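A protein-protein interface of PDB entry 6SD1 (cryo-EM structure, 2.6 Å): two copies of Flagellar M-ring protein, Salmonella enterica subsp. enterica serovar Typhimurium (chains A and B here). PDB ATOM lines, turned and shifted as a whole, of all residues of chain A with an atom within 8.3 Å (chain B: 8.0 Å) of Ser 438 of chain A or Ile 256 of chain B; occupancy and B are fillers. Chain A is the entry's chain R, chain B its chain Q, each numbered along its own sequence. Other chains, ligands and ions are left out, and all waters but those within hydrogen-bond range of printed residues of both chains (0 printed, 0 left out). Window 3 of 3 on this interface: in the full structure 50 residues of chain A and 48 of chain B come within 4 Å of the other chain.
Position printed for both chains: 391.
Of the printed residues of chain B, His 263 of chain A touches Ile 252 and Pro 255. Of the printed residues of chain B, Val 390 of chain A touches Ile 252, Ile 256 and Leu 415. Printed residues of chain B within 4 Å of Pro 436 of chain A: Pro 255. Of chain B, only Pro 255 and Ile 256 come within 4 Å of Ser 438 of chain A. Of the printed residues of chain A, Pro 255 of chain B touches His 263 (3.7 Å), Pro 436 (3.9 Å), Phe 437 (3.2 Å) and Ser 438 (3.5 Å). Of the printed residues of chain A, Ile 256 of chain B touches Val 390 (3.97 Å), Ser 435 (3.2 Å) and Ser 438 (3.4 Å). Val 391 of chain B touches none of the printed residues of chain A. The nearest printed residue of chain A that does not touch Ile 256 of chain B is Pro 436 of chain A (4.01 Å). The nearest printed residue of chain B that does not touch Asn 431 of chain A is Gln 411 of chain B (4.8 Å).
The backbone NH (N) of Val 390 of chain A sits at hydrogen-bond distance from the backbone carbonyl oxygen (O) of His 263 of chain A (2.9 Å). The backbone NH (N) of Val 389 of chain A sits at hydrogen-bond distance from the backbone carbonyl oxygen (O) of Asn 431 of chain A. The backbone NH (N) of Val 433 of chain A is in hydrogen-bond range of the backbone carbonyl oxygen (O) of Val 389 of chain A, 3.1 Å away. The backbone NH (N) of Val 391 of chain A lies within hydrogen-bond range of the backbone carbonyl oxygen (O) of Val 433 of chain A (3.2 Å). The backbone carbonyl oxygen of Val 391 of chain A sits at hydrogen-bond distance from the backbone NH of Ser 435 of chain A (3.3 Å). The backbone NH (N) of Phe 437 of chain A is in hydrogen-bond range of the side-chain amide oxygen (OD1) of Asn 392 of chain A (3.2 Å).
CD1 of Ile 252 of chain B touches O of His 263 of chain A (3.6 Å). His 263 of chain A touches Pro 255 of chain B. CG2 of Val 390 of chain A touches CD1 of Ile 252 of chain B (3.998 Å). Val 390 of chain A touches Ile 256 of chain B. CG1 of Val 390 of chain A touches CD1 of Leu 415 of chain B, 3.6 Å away. CG1 of Ile 256 of chain B touches OG of Ser 435 of chain A, 3.2 Å away. Gln 411 of chain B touches Ser 435 of chain A (NE2 to CB, 3.6 Å). Pro 255 of chain B touches Pro 436 of chain A. Phe 437 of chain A touches Pro 255 of chain B. Ser 438 of chain A touches Pro 255 of chain B.
O of Ile 256 of chain B is in hydrogen-bond range of OG of Ser 438 of chain A, at 3.4 Å. OD1 of Asp 414 of chain B is in hydrogen-bond range of ND2 of Asn 431 of chain A, 2.8 Å away.
Of the 12 printed residues of chain A, 8 touch a printed residue of chain B. Printed residues of chain A that touch a printed residue of chain B: His 263, Val 390, Asn 431, Val 433, Ser 435, Pro 436, Phe 437 and Ser 438. Hydrophobic or aromatic side chains of chain A that line the printed part of chain B: His 263, Val 390, Val 433 and Phe 437. Of the 21 printed residues of chain B, 6 touch a printed residue of chain A. Hydrophobic or aromatic side chains of chain B that line the printed part of chain A: Ile 252, Pro 255, Ile 256 and Leu 415. Among the printed residues, no Asp or Glu carboxylate lies within 4 Å of a Lys or Arg side-chain nitrogen of the other chain.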
ATOM      1  N   HIS A 263      20.018 -24.645 -20.367  1.00  0.00           N
ATOM      2  CA  HIS A 263      19.340 -23.509 -20.972  1.00  0.00           C
ATOM      3  C   HIS A 263      19.702 -23.444 -22.443  1.00  0.00           C
ATOM      4  O   HIS A 263      20.864 -23.636 -22.814  1.00  0.00           O
ATOM      5  CB  HIS A 263      19.714 -22.194 -20.280  1.00  0.00           C
ATOM      6  CG  HIS A 263      19.171 -22.067 -18.893  1.00  0.00           C
ATOM      7  ND1 HIS A 263      17.887 -21.644 -18.633  1.00  0.00           N
ATOM      8  CD2 HIS A 263      19.738 -22.312 -17.689  1.00  0.00           C
ATOM      9  CE1 HIS A 263      17.685 -21.632 -17.327  1.00  0.00           C
ATOM     10  NE2 HIS A 263      18.793 -22.034 -16.732  1.00  0.00           N
ATOM     11  N   VAL A 389      23.493 -23.681 -26.267  1.00  0.00           N
ATOM     12  CA  VAL A 389      23.069 -24.489 -25.132  1.00  0.00           C
ATOM     13  C   VAL A 389      24.138 -24.402 -24.054  1.00  0.00           C
ATOM     14  O   VAL A 389      25.328 -24.567 -24.339  1.00  0.00           O
ATOM     15  CB  VAL A 389      22.822 -25.955 -25.537  1.00  0.00           C
ATOM     16  CG1 VAL A 389      22.497 -26.799 -24.315  1.00  0.00           C
ATOM     17  CG2 VAL A 389      21.707 -26.045 -26.561  1.00  0.00           C
ATOM     18  N   VAL A 390      23.712 -24.141 -22.822  1.00  0.00           N
ATOM     19  CA  VAL A 390      24.590 -24.160 -21.659  1.00  0.00           C
ATOM     20  C   VAL A 390      24.071 -25.213 -20.692  1.00  0.00           C
ATOM     21  O   VAL A 390      22.862 -25.295 -20.443  1.00  0.00           O
ATOM     22  CB  VAL A 390      24.682 -22.777 -20.987  1.00  0.00           C
ATOM     23  CG1 VAL A 390      25.379 -21.797 -21.902  1.00  0.00           C
ATOM     24  CG2 VAL A 390      23.304 -22.255 -20.624  1.00  0.00           C
ATOM     25  N   VAL A 391      24.977 -26.029 -20.161  1.00  0.00           N
ATOM     26  CA  VAL A 391      24.636 -27.081 -19.213  1.00  0.00           C
ATOM     27  C   VAL A 391      25.449 -26.876 -17.944  1.00  0.00           C
ATOM     28  O   VAL A 391      26.636 -26.541 -17.999  1.00  0.00           O
ATOM     29  CB  VAL A 391      24.877 -28.486 -19.804  1.00  0.00           C
ATOM     30  CG1 VAL A 391      23.763 -28.848 -20.764  1.00  0.00           C
ATOM     31  CG2 VAL A 391      26.220 -28.547 -20.509  1.00  0.00           C
ATOM     32  N   ASN A 392      24.800 -27.074 -16.800  1.00  0.00           N
ATOM     33  CA  ASN A 392      25.438 -26.867 -15.510  1.00  0.00           C
ATOM     34  C   ASN A 392      26.470 -27.960 -15.241  1.00  0.00           C
ATOM     35  O   ASN A 392      26.467 -29.028 -15.859  1.00  0.00           O
ATOM     36  CB  ASN A 392      24.386 -26.850 -14.402  1.00  0.00           C
ATOM     37  CG  ASN A 392      24.859 -26.137 -13.157  1.00  0.00           C
ATOM     38  OD1 ASN A 392      26.058 -25.994 -12.926  1.00  0.00           O
ATOM     39  ND2 ASN A 392      23.914 -25.689 -12.340  1.00  0.00           N
ATOM     40  N   ASN A 431      26.221 -24.446 -30.528  1.00  0.00           N
ATOM     41  CA  ASN A 431      27.275 -24.269 -29.536  1.00  0.00           C
ATOM     42  C   ASN A 431      26.770 -24.755 -28.191  1.00  0.00           C
ATOM     43  O   ASN A 431      25.803 -24.208 -27.655  1.00  0.00           O
ATOM     44  CB  ASN A 431      27.716 -22.809 -29.439  1.00  0.00           C
ATOM     45  CG  ASN A 431      29.108 -22.662 -28.870  1.00  0.00           C
ATOM     46  OD1 ASN A 431      30.013 -23.423 -29.208  1.00  0.00           O
ATOM     47  ND2 ASN A 431      29.280 -21.698 -27.979  1.00  0.00           N
ATOM     48  N   VAL A 433      28.283 -25.339 -24.414  1.00  0.00           N
ATOM     49  CA  VAL A 433      29.379 -25.157 -23.476  1.00  0.00           C
ATOM     50  C   VAL A 433      28.954 -25.718 -22.129  1.00  0.00           C
ATOM     51  O   VAL A 433      27.762 -25.815 -21.819  1.00  0.00           O
ATOM     52  CB  VAL A 433      29.800 -23.677 -23.338  1.00  0.00           C
ATOM     53  CG1 VAL A 433      30.036 -23.060 -24.704  1.00  0.00           C
ATOM     54  CG2 VAL A 433      28.761 -22.900 -22.560  1.00  0.00           C
ATOM     55  N   ASN A 434      29.944 -26.097 -21.331  1.00  0.00           N
ATOM     56  CA  ASN A 434      29.719 -26.612 -19.989  1.00  0.00           C
ATOM     57  C   ASN A 434      30.383 -25.671 -18.993  1.00  0.00           C
ATOM     58  O   ASN A 434      31.610 -25.528 -18.992  1.00  0.00           O
ATOM     59  CB  ASN A 434      30.268 -28.030 -19.854  1.00  0.00           C
ATOM     60  CG  ASN A 434      29.733 -28.747 -18.637  1.00  0.00           C
ATOM     61  OD1 ASN A 434      28.701 -28.374 -18.085  1.00  0.00           O
ATOM     62  ND2 ASN A 434      30.437 -29.781 -18.210  1.00  0.00           N
ATOM     63  N   SER A 435      29.574 -25.027 -18.154  1.00  0.00           N
ATOM     64  CA  SER A 435      30.090 -24.064 -17.201  1.00  0.00           C
ATOM     65  C   SER A 435      29.187 -24.044 -15.978  1.00  0.00           C
ATOM     66  O   SER A 435      27.976 -24.272 -16.112  1.00  0.00           O
ATOM     67  CB  SER A 435      30.174 -22.661 -17.807  1.00  0.00           C
ATOM     68  OG  SER A 435      28.931 -21.996 -17.697  1.00  0.00           O
ATOM     69  N   PRO A 436      29.732 -23.777 -14.793  1.00  0.00           N
ATOM     70  CA  PRO A 436      28.897 -23.767 -13.588  1.00  0.00           C
ATOM     71  C   PRO A 436      27.929 -22.597 -13.600  1.00  0.00           C
ATOM     72  O   PRO A 436      28.241 -21.515 -14.103  1.00  0.00           O
ATOM     73  CB  PRO A 436      29.915 -23.643 -12.451  1.00  0.00           C
ATOM     74  CG  PRO A 436      31.102 -23.010 -13.073  1.00  0.00           C
ATOM     75  CD  PRO A 436      31.142 -23.472 -14.496  1.00  0.00           C
ATOM     76  N   PHE A 437      26.747 -22.822 -13.038  1.00  0.00           N
ATOM     77  CA  PHE A 437      25.693 -21.819 -13.060  1.00  0.00           C
ATOM     78  C   PHE A 437      25.880 -20.840 -11.904  1.00  0.00           C
ATOM     79  O   PHE A 437      26.974 -20.683 -11.356  1.00  0.00           O
ATOM     80  CB  PHE A 437      24.321 -22.485 -13.021  1.00  0.00           C
ATOM     81  CG  PHE A 437      23.847 -22.978 -14.357  1.00  0.00           C
ATOM     82  CD1 PHE A 437      24.738 -23.168 -15.399  1.00  0.00           C
ATOM     83  CD2 PHE A 437      22.509 -23.252 -14.570  1.00  0.00           C
ATOM     84  CE1 PHE A 437      24.303 -23.621 -16.623  1.00  0.00           C
ATOM     85  CE2 PHE A 437      22.069 -23.707 -15.793  1.00  0.00           C
ATOM     86  CZ  PHE A 437      22.967 -23.891 -16.821  1.00  0.00           C
ATOM     87  N   SER A 438      24.802 -20.166 -11.521  1.00  0.00           N
ATOM     88  CA  SER A 438      24.860 -19.161 -10.470  1.00  0.00           C
ATOM     89  C   SER A 438      23.575 -19.163  -9.651  1.00  0.00           C
ATOM     90  O   SER A 438      22.768 -18.241  -9.745  1.00  0.00           O
ATOM     91  CB  SER A 438      25.108 -17.776 -11.070  1.00  0.00           C
ATOM     92  OG  SER A 438      26.368 -17.719 -11.714  1.00  0.00           O
ATOM     93  N   GLU B 250      21.050 -11.908 -23.099  1.00  0.00           N
ATOM     94  CA  GLU B 250      21.023 -11.851 -21.645  1.00  0.00           C
ATOM     95  C   GLU B 250      20.337 -13.057 -21.020  1.00  0.00           C
ATOM     96  O   GLU B 250      20.363 -13.193 -19.793  1.00  0.00           O
ATOM     97  CB  GLU B 250      20.335 -10.566 -21.186  1.00  0.00           C
ATOM     98  CG  GLU B 250      21.140  -9.309 -21.457  1.00  0.00           C
ATOM     99  CD  GLU B 250      20.265  -8.118 -21.786  1.00  0.00           C
ATOM    100  OE1 GLU B 250      19.050  -8.311 -21.991  1.00  0.00           O
ATOM    101  OE2 GLU B 250      20.795  -6.987 -21.839  1.00  0.00           O
ATOM    102  N   ALA B 251      19.722 -13.927 -21.820  1.00  0.00           N
ATOM    103  CA  ALA B 251      19.124 -15.148 -21.301  1.00  0.00           C
ATOM    104  C   ALA B 251      20.064 -16.340 -21.368  1.00  0.00           C
ATOM    105  O   ALA B 251      19.894 -17.288 -20.593  1.00  0.00           O
ATOM    106  CB  ALA B 251      17.837 -15.479 -22.059  1.00  0.00           C
ATOM    107  N   ILE B 252      21.046 -16.318 -22.268  1.00  0.00           N
ATOM    108  CA  ILE B 252      22.015 -17.403 -22.346  1.00  0.00           C
ATOM    109  C   ILE B 252      23.303 -17.085 -21.597  1.00  0.00           C
ATOM    110  O   ILE B 252      24.107 -17.995 -21.352  1.00  0.00           O
ATOM    111  CB  ILE B 252      22.325 -17.753 -23.813  1.00  0.00           C
ATOM    112  CG1 ILE B 252      22.708 -19.228 -23.939  1.00  0.00           C
ATOM    113  CG2 ILE B 252      23.429 -16.866 -24.358  1.00  0.00           C
ATOM    114  CD1 ILE B 252      21.592 -20.176 -23.579  1.00  0.00           C
ATOM    115  N   LEU B 253      23.522 -15.825 -21.220  1.00  0.00           N
ATOM    116  CA  LEU B 253      24.698 -15.447 -20.452  1.00  0.00           C
ATOM    117  C   LEU B 253      24.404 -15.238 -18.974  1.00  0.00           C
ATOM    118  O   LEU B 253      25.334 -15.285 -18.163  1.00  0.00           O
ATOM    119  CB  LEU B 253      25.322 -14.170 -21.026  1.00  0.00           C
ATOM    120  CG  LEU B 253      25.909 -14.278 -22.433  1.00  0.00           C
ATOM    121  CD1 LEU B 253      26.529 -12.958 -22.850  1.00  0.00           C
ATOM    122  CD2 LEU B 253      26.931 -15.399 -22.508  1.00  0.00           C
ATOM    123  N   SER B 254      23.145 -15.008 -18.609  1.00  0.00           N
ATOM    124  CA  SER B 254      22.801 -14.888 -17.197  1.00  0.00           C
ATOM    125  C   SER B 254      23.065 -16.156 -16.387  1.00  0.00           C
ATOM    126  O   SER B 254      23.489 -16.021 -15.226  1.00  0.00           O
ATOM    127  CB  SER B 254      21.333 -14.459 -17.056  1.00  0.00           C
ATOM    128  OG  SER B 254      21.099 -13.230 -17.718  1.00  0.00           O
ATOM    129  N   PRO B 255      22.831 -17.374 -16.891  1.00  0.00           N
ATOM    130  CA  PRO B 255      23.218 -18.552 -16.102  1.00  0.00           C
ATOM    131  C   PRO B 255      24.715 -18.674 -15.886  1.00  0.00           C
ATOM    132  O   PRO B 255      25.133 -19.309 -14.913  1.00  0.00           O
ATOM    133  CB  PRO B 255      22.673 -19.723 -16.931  1.00  0.00           C
ATOM    134  CG  PRO B 255      21.551 -19.141 -17.694  1.00  0.00           C
ATOM    135  CD  PRO B 255      22.003 -17.759 -18.048  1.00  0.00           C
ATOM    136  N   ILE B 256      25.536 -18.083 -16.750  1.00  0.00           N
ATOM    137  CA  ILE B 256      26.983 -18.250 -16.634  1.00  0.00           C
ATOM    138  C   ILE B 256      27.576 -17.210 -15.693  1.00  0.00           C
ATOM    139  O   ILE B 256      28.124 -17.543 -14.636  1.00  0.00           O
ATOM    140  CB  ILE B 256      27.648 -18.192 -18.020  1.00  0.00           C
ATOM    141  CG1 ILE B 256      27.298 -19.439 -18.827  1.00  0.00           C
ATOM    142  CG2 ILE B 256      29.157 -18.055 -17.879  1.00  0.00           C
ATOM    143  CD1 ILE B 256      28.140 -19.609 -20.061  1.00  0.00           C
ATOM    144  N   VAL B 257      27.481 -15.934 -16.065  1.00  0.00           N
ATOM    145  CA  VAL B 257      28.173 -14.886 -15.324  1.00  0.00           C
ATOM    146  C   VAL B 257      27.352 -14.320 -14.172  1.00  0.00           C
ATOM    147  O   VAL B 257      27.930 -13.738 -13.244  1.00  0.00           O
ATOM    148  CB  VAL B 257      28.594 -13.745 -16.267  1.00  0.00           C
ATOM    149  CG1 VAL B 257      29.531 -14.267 -17.338  1.00  0.00           C
ATOM    150  CG2 VAL B 257      27.374 -13.092 -16.894  1.00  0.00           C
ATOM    151  N   GLY B 258      26.035 -14.474 -14.197  1.00  0.00           N
ATOM    152  CA  GLY B 258      25.176 -13.949 -13.157  1.00  0.00           C
ATOM    153  C   GLY B 258      23.948 -13.272 -13.732  1.00  0.00           C
ATOM    154  O   GLY B 258      23.887 -12.907 -14.904  1.00  0.00           O
ATOM    155  N   ASN B 259      22.955 -13.103 -12.856  1.00  0.00           N
ATOM    156  CA  ASN B 259      21.672 -12.556 -13.281  1.00  0.00           C
ATOM    157  C   ASN B 259      21.802 -11.135 -13.814  1.00  0.00           C
ATOM    158  O   ASN B 259      21.086 -10.759 -14.748  1.00  0.00           O
ATOM    159  CB  ASN B 259      20.678 -12.594 -12.121  1.00  0.00           C
ATOM    160  CG  ASN B 259      19.356 -11.943 -12.467  1.00  0.00           C
ATOM    161  OD1 ASN B 259      18.737 -12.267 -13.480  1.00  0.00           O
ATOM    162  ND2 ASN B 259      18.918 -11.013 -11.628  1.00  0.00           N
ATOM    163  N   ASN B 261      25.124  -9.506 -14.224  1.00  0.00           N
ATOM    164  CA  ASN B 261      26.522  -9.235 -14.525  1.00  0.00           C
ATOM    165  C   ASN B 261      26.805  -9.211 -16.020  1.00  0.00           C
ATOM    166  O   ASN B 261      27.945  -9.462 -16.429  1.00  0.00           O
ATOM    167  CB  ASN B 261      27.416 -10.266 -13.835  1.00  0.00           C
ATOM    168  CG  ASN B 261      27.325 -10.194 -12.324  1.00  0.00           C
ATOM    169  OD1 ASN B 261      28.057  -9.439 -11.685  1.00  0.00           O
ATOM    170  ND2 ASN B 261      26.425 -10.976 -11.746  1.00  0.00           N
ATOM    171  N   VAL B 262      25.804  -8.916 -16.841  1.00  0.00           N
ATOM    172  CA  VAL B 262      25.989  -8.837 -18.286  1.00  0.00           C
ATOM    173  C   VAL B 262      24.993  -7.832 -18.845  1.00  0.00           C
ATOM    174  O   VAL B 262      23.836  -7.776 -18.418  1.00  0.00           O
ATOM    175  CB  VAL B 262      25.841 -10.224 -18.954  1.00  0.00           C
ATOM    176  CG1 VAL B 262      24.463 -10.816 -18.693  1.00  0.00           C
ATOM    177  CG2 VAL B 262      26.118 -10.132 -20.444  1.00  0.00           C
ATOM    178  N   VAL B 391      30.562  -7.664 -19.617  1.00  0.00           N
ATOM    179  CA  VAL B 391      30.387  -8.623 -18.534  1.00  0.00           C
ATOM    180  C   VAL B 391      31.197  -8.156 -17.334  1.00  0.00           C
ATOM    181  O   VAL B 391      32.305  -7.629 -17.484  1.00  0.00           O
ATOM    182  CB  VAL B 391      30.791 -10.050 -18.959  1.00  0.00           C
ATOM    183  CG1 VAL B 391      29.793 -10.602 -19.958  1.00  0.00           C
ATOM    184  CG2 VAL B 391      32.185 -10.055 -19.556  1.00  0.00           C
ATOM    185  N   LYS B 394      34.603 -10.632 -11.246  1.00  0.00           N
ATOM    186  CA  LYS B 394      34.190 -11.510 -10.160  1.00  0.00           C
ATOM    187  C   LYS B 394      35.224 -11.513  -9.040  1.00  0.00           C
ATOM    188  O   LYS B 394      36.216 -10.786  -9.098  1.00  0.00           O
ATOM    189  CB  LYS B 394      33.967 -12.931 -10.679  1.00  0.00           C
ATOM    190  CG  LYS B 394      35.246 -13.652 -11.063  1.00  0.00           C
ATOM    191  CD  LYS B 394      34.948 -14.993 -11.708  1.00  0.00           C
ATOM    192  CE  LYS B 394      34.313 -15.954 -10.718  1.00  0.00           C
ATOM    193  NZ  LYS B 394      34.116 -17.305 -11.312  1.00  0.00           N
ATOM    194  N   LEU B 404      37.843 -12.325 -15.826  1.00  0.00           N
ATOM    195  CA  LEU B 404      37.491 -13.668 -16.261  1.00  0.00           C
ATOM    196  C   LEU B 404      38.584 -14.229 -17.162  1.00  0.00           C
ATOM    197  O   LEU B 404      39.180 -13.514 -17.970  1.00  0.00           O
ATOM    198  CB  LEU B 404      36.153 -13.653 -17.001  1.00  0.00           C
ATOM    199  CG  LEU B 404      34.883 -13.905 -16.185  1.00  0.00           C
ATOM    200  CD1 LEU B 404      34.754 -12.917 -15.040  1.00  0.00           C
ATOM    201  CD2 LEU B 404      33.661 -13.839 -17.085  1.00  0.00           C
ATOM    202  N   GLN B 408      36.954 -18.627 -20.328  1.00  0.00           N
ATOM    203  CA  GLN B 408      35.558 -18.257 -20.131  1.00  0.00           C
ATOM    204  C   GLN B 408      35.119 -17.169 -21.102  1.00  0.00           C
ATOM    205  O   GLN B 408      33.987 -17.204 -21.595  1.00  0.00           O
ATOM    206  CB  GLN B 408      35.336 -17.805 -18.688  1.00  0.00           C
ATOM    207  CG  GLN B 408      33.875 -17.625 -18.317  1.00  0.00           C
ATOM    208  CD  GLN B 408      33.665 -17.518 -16.821  1.00  0.00           C
ATOM    209  OE1 GLN B 408      34.575 -17.775 -16.034  1.00  0.00           O
ATOM    210  NE2 GLN B 408      32.459 -17.136 -16.420  1.00  0.00           N
ATOM    211  N   MET B 409      35.992 -16.203 -21.395  1.00  0.00           N
ATOM    212  CA  MET B 409      35.625 -15.146 -22.328  1.00  0.00           C
ATOM    213  C   MET B 409      35.512 -15.669 -23.753  1.00  0.00           C
ATOM    214  O   MET B 409      34.754 -15.113 -24.556  1.00  0.00           O
ATOM    215  CB  MET B 409      36.639 -14.004 -22.258  1.00  0.00           C
ATOM    216  CG  MET B 409      36.575 -13.206 -20.968  1.00  0.00           C
ATOM    217  SD  MET B 409      34.962 -12.446 -20.711  1.00  0.00           S
ATOM    218  CE  MET B 409      34.910 -11.294 -22.079  1.00  0.00           C
ATOM    219  N   GLN B 411      34.328 -18.681 -24.496  1.00  0.00           N
ATOM    220  CA  GLN B 411      33.041 -19.359 -24.565  1.00  0.00           C
ATOM    221  C   GLN B 411      31.882 -18.407 -24.306  1.00  0.00           C
ATOM    222  O   GLN B 411      30.723 -18.789 -24.484  1.00  0.00           O
ATOM    223  CB  GLN B 411      33.000 -20.527 -23.577  1.00  0.00           C
ATOM    224  CG  GLN B 411      32.701 -20.133 -22.144  1.00  0.00           C
ATOM    225  CD  GLN B 411      33.086 -21.216 -21.158  1.00  0.00           C
ATOM    226  OE1 GLN B 411      33.844 -22.127 -21.486  1.00  0.00           O
ATOM    227  NE2 GLN B 411      32.562 -21.123 -19.942  1.00  0.00           N
ATOM    228  N   ILE B 412      32.166 -17.176 -23.879  1.00  0.00           N
ATOM    229  CA  ILE B 412      31.119 -16.162 -23.803  1.00  0.00           C
ATOM    230  C   ILE B 412      30.909 -15.530 -25.171  1.00  0.00           C
ATOM    231  O   ILE B 412      29.784 -15.177 -25.548  1.00  0.00           O
ATOM    232  CB  ILE B 412      31.470 -15.112 -22.731  1.00  0.00           C
ATOM    233  CG1 ILE B 412      31.186 -15.662 -21.335  1.00  0.00           C
ATOM    234  CG2 ILE B 412      30.701 -13.820 -22.951  1.00  0.00           C
ATOM    235  CD1 ILE B 412      31.678 -14.767 -20.230  1.00  0.00           C
ATOM    236  N   ASP B 414      31.366 -16.994 -28.186  1.00  0.00           N
ATOM    237  CA  ASP B 414      30.768 -17.879 -29.181  1.00  0.00           C
ATOM    238  C   ASP B 414      29.319 -18.214 -28.841  1.00  0.00           C
ATOM    239  O   ASP B 414      28.541 -18.576 -29.730  1.00  0.00           O
ATOM    240  CB  ASP B 414      31.611 -19.143 -29.338  1.00  0.00           C
ATOM    241  CG  ASP B 414      31.774 -19.910 -28.044  1.00  0.00           C
ATOM    242  OD1 ASP B 414      30.996 -19.681 -27.096  1.00  0.00           O
ATOM    243  OD2 ASP B 414      32.692 -20.754 -27.973  1.00  0.00           O
ATOM    244  N   LEU B 415      28.937 -18.107 -27.568  1.00  0.00           N
ATOM    245  CA  LEU B 415      27.522 -18.225 -27.223  1.00  0.00           C
ATOM    246  C   LEU B 415      26.745 -16.998 -27.673  1.00  0.00           C
ATOM    247  O   LEU B 415      25.669 -17.121 -28.266  1.00  0.00           O
ATOM    248  CB  LEU B 415      27.347 -18.428 -25.723  1.00  0.00           C
ATOM    249  CG  LEU B 415      27.789 -19.753 -25.118  1.00  0.00           C
ATOM    250  CD1 LEU B 415      27.722 -19.636 -23.617  1.00  0.00           C
ATOM    251  CD2 LEU B 415      26.912 -20.887 -25.616  1.00  0.00           C
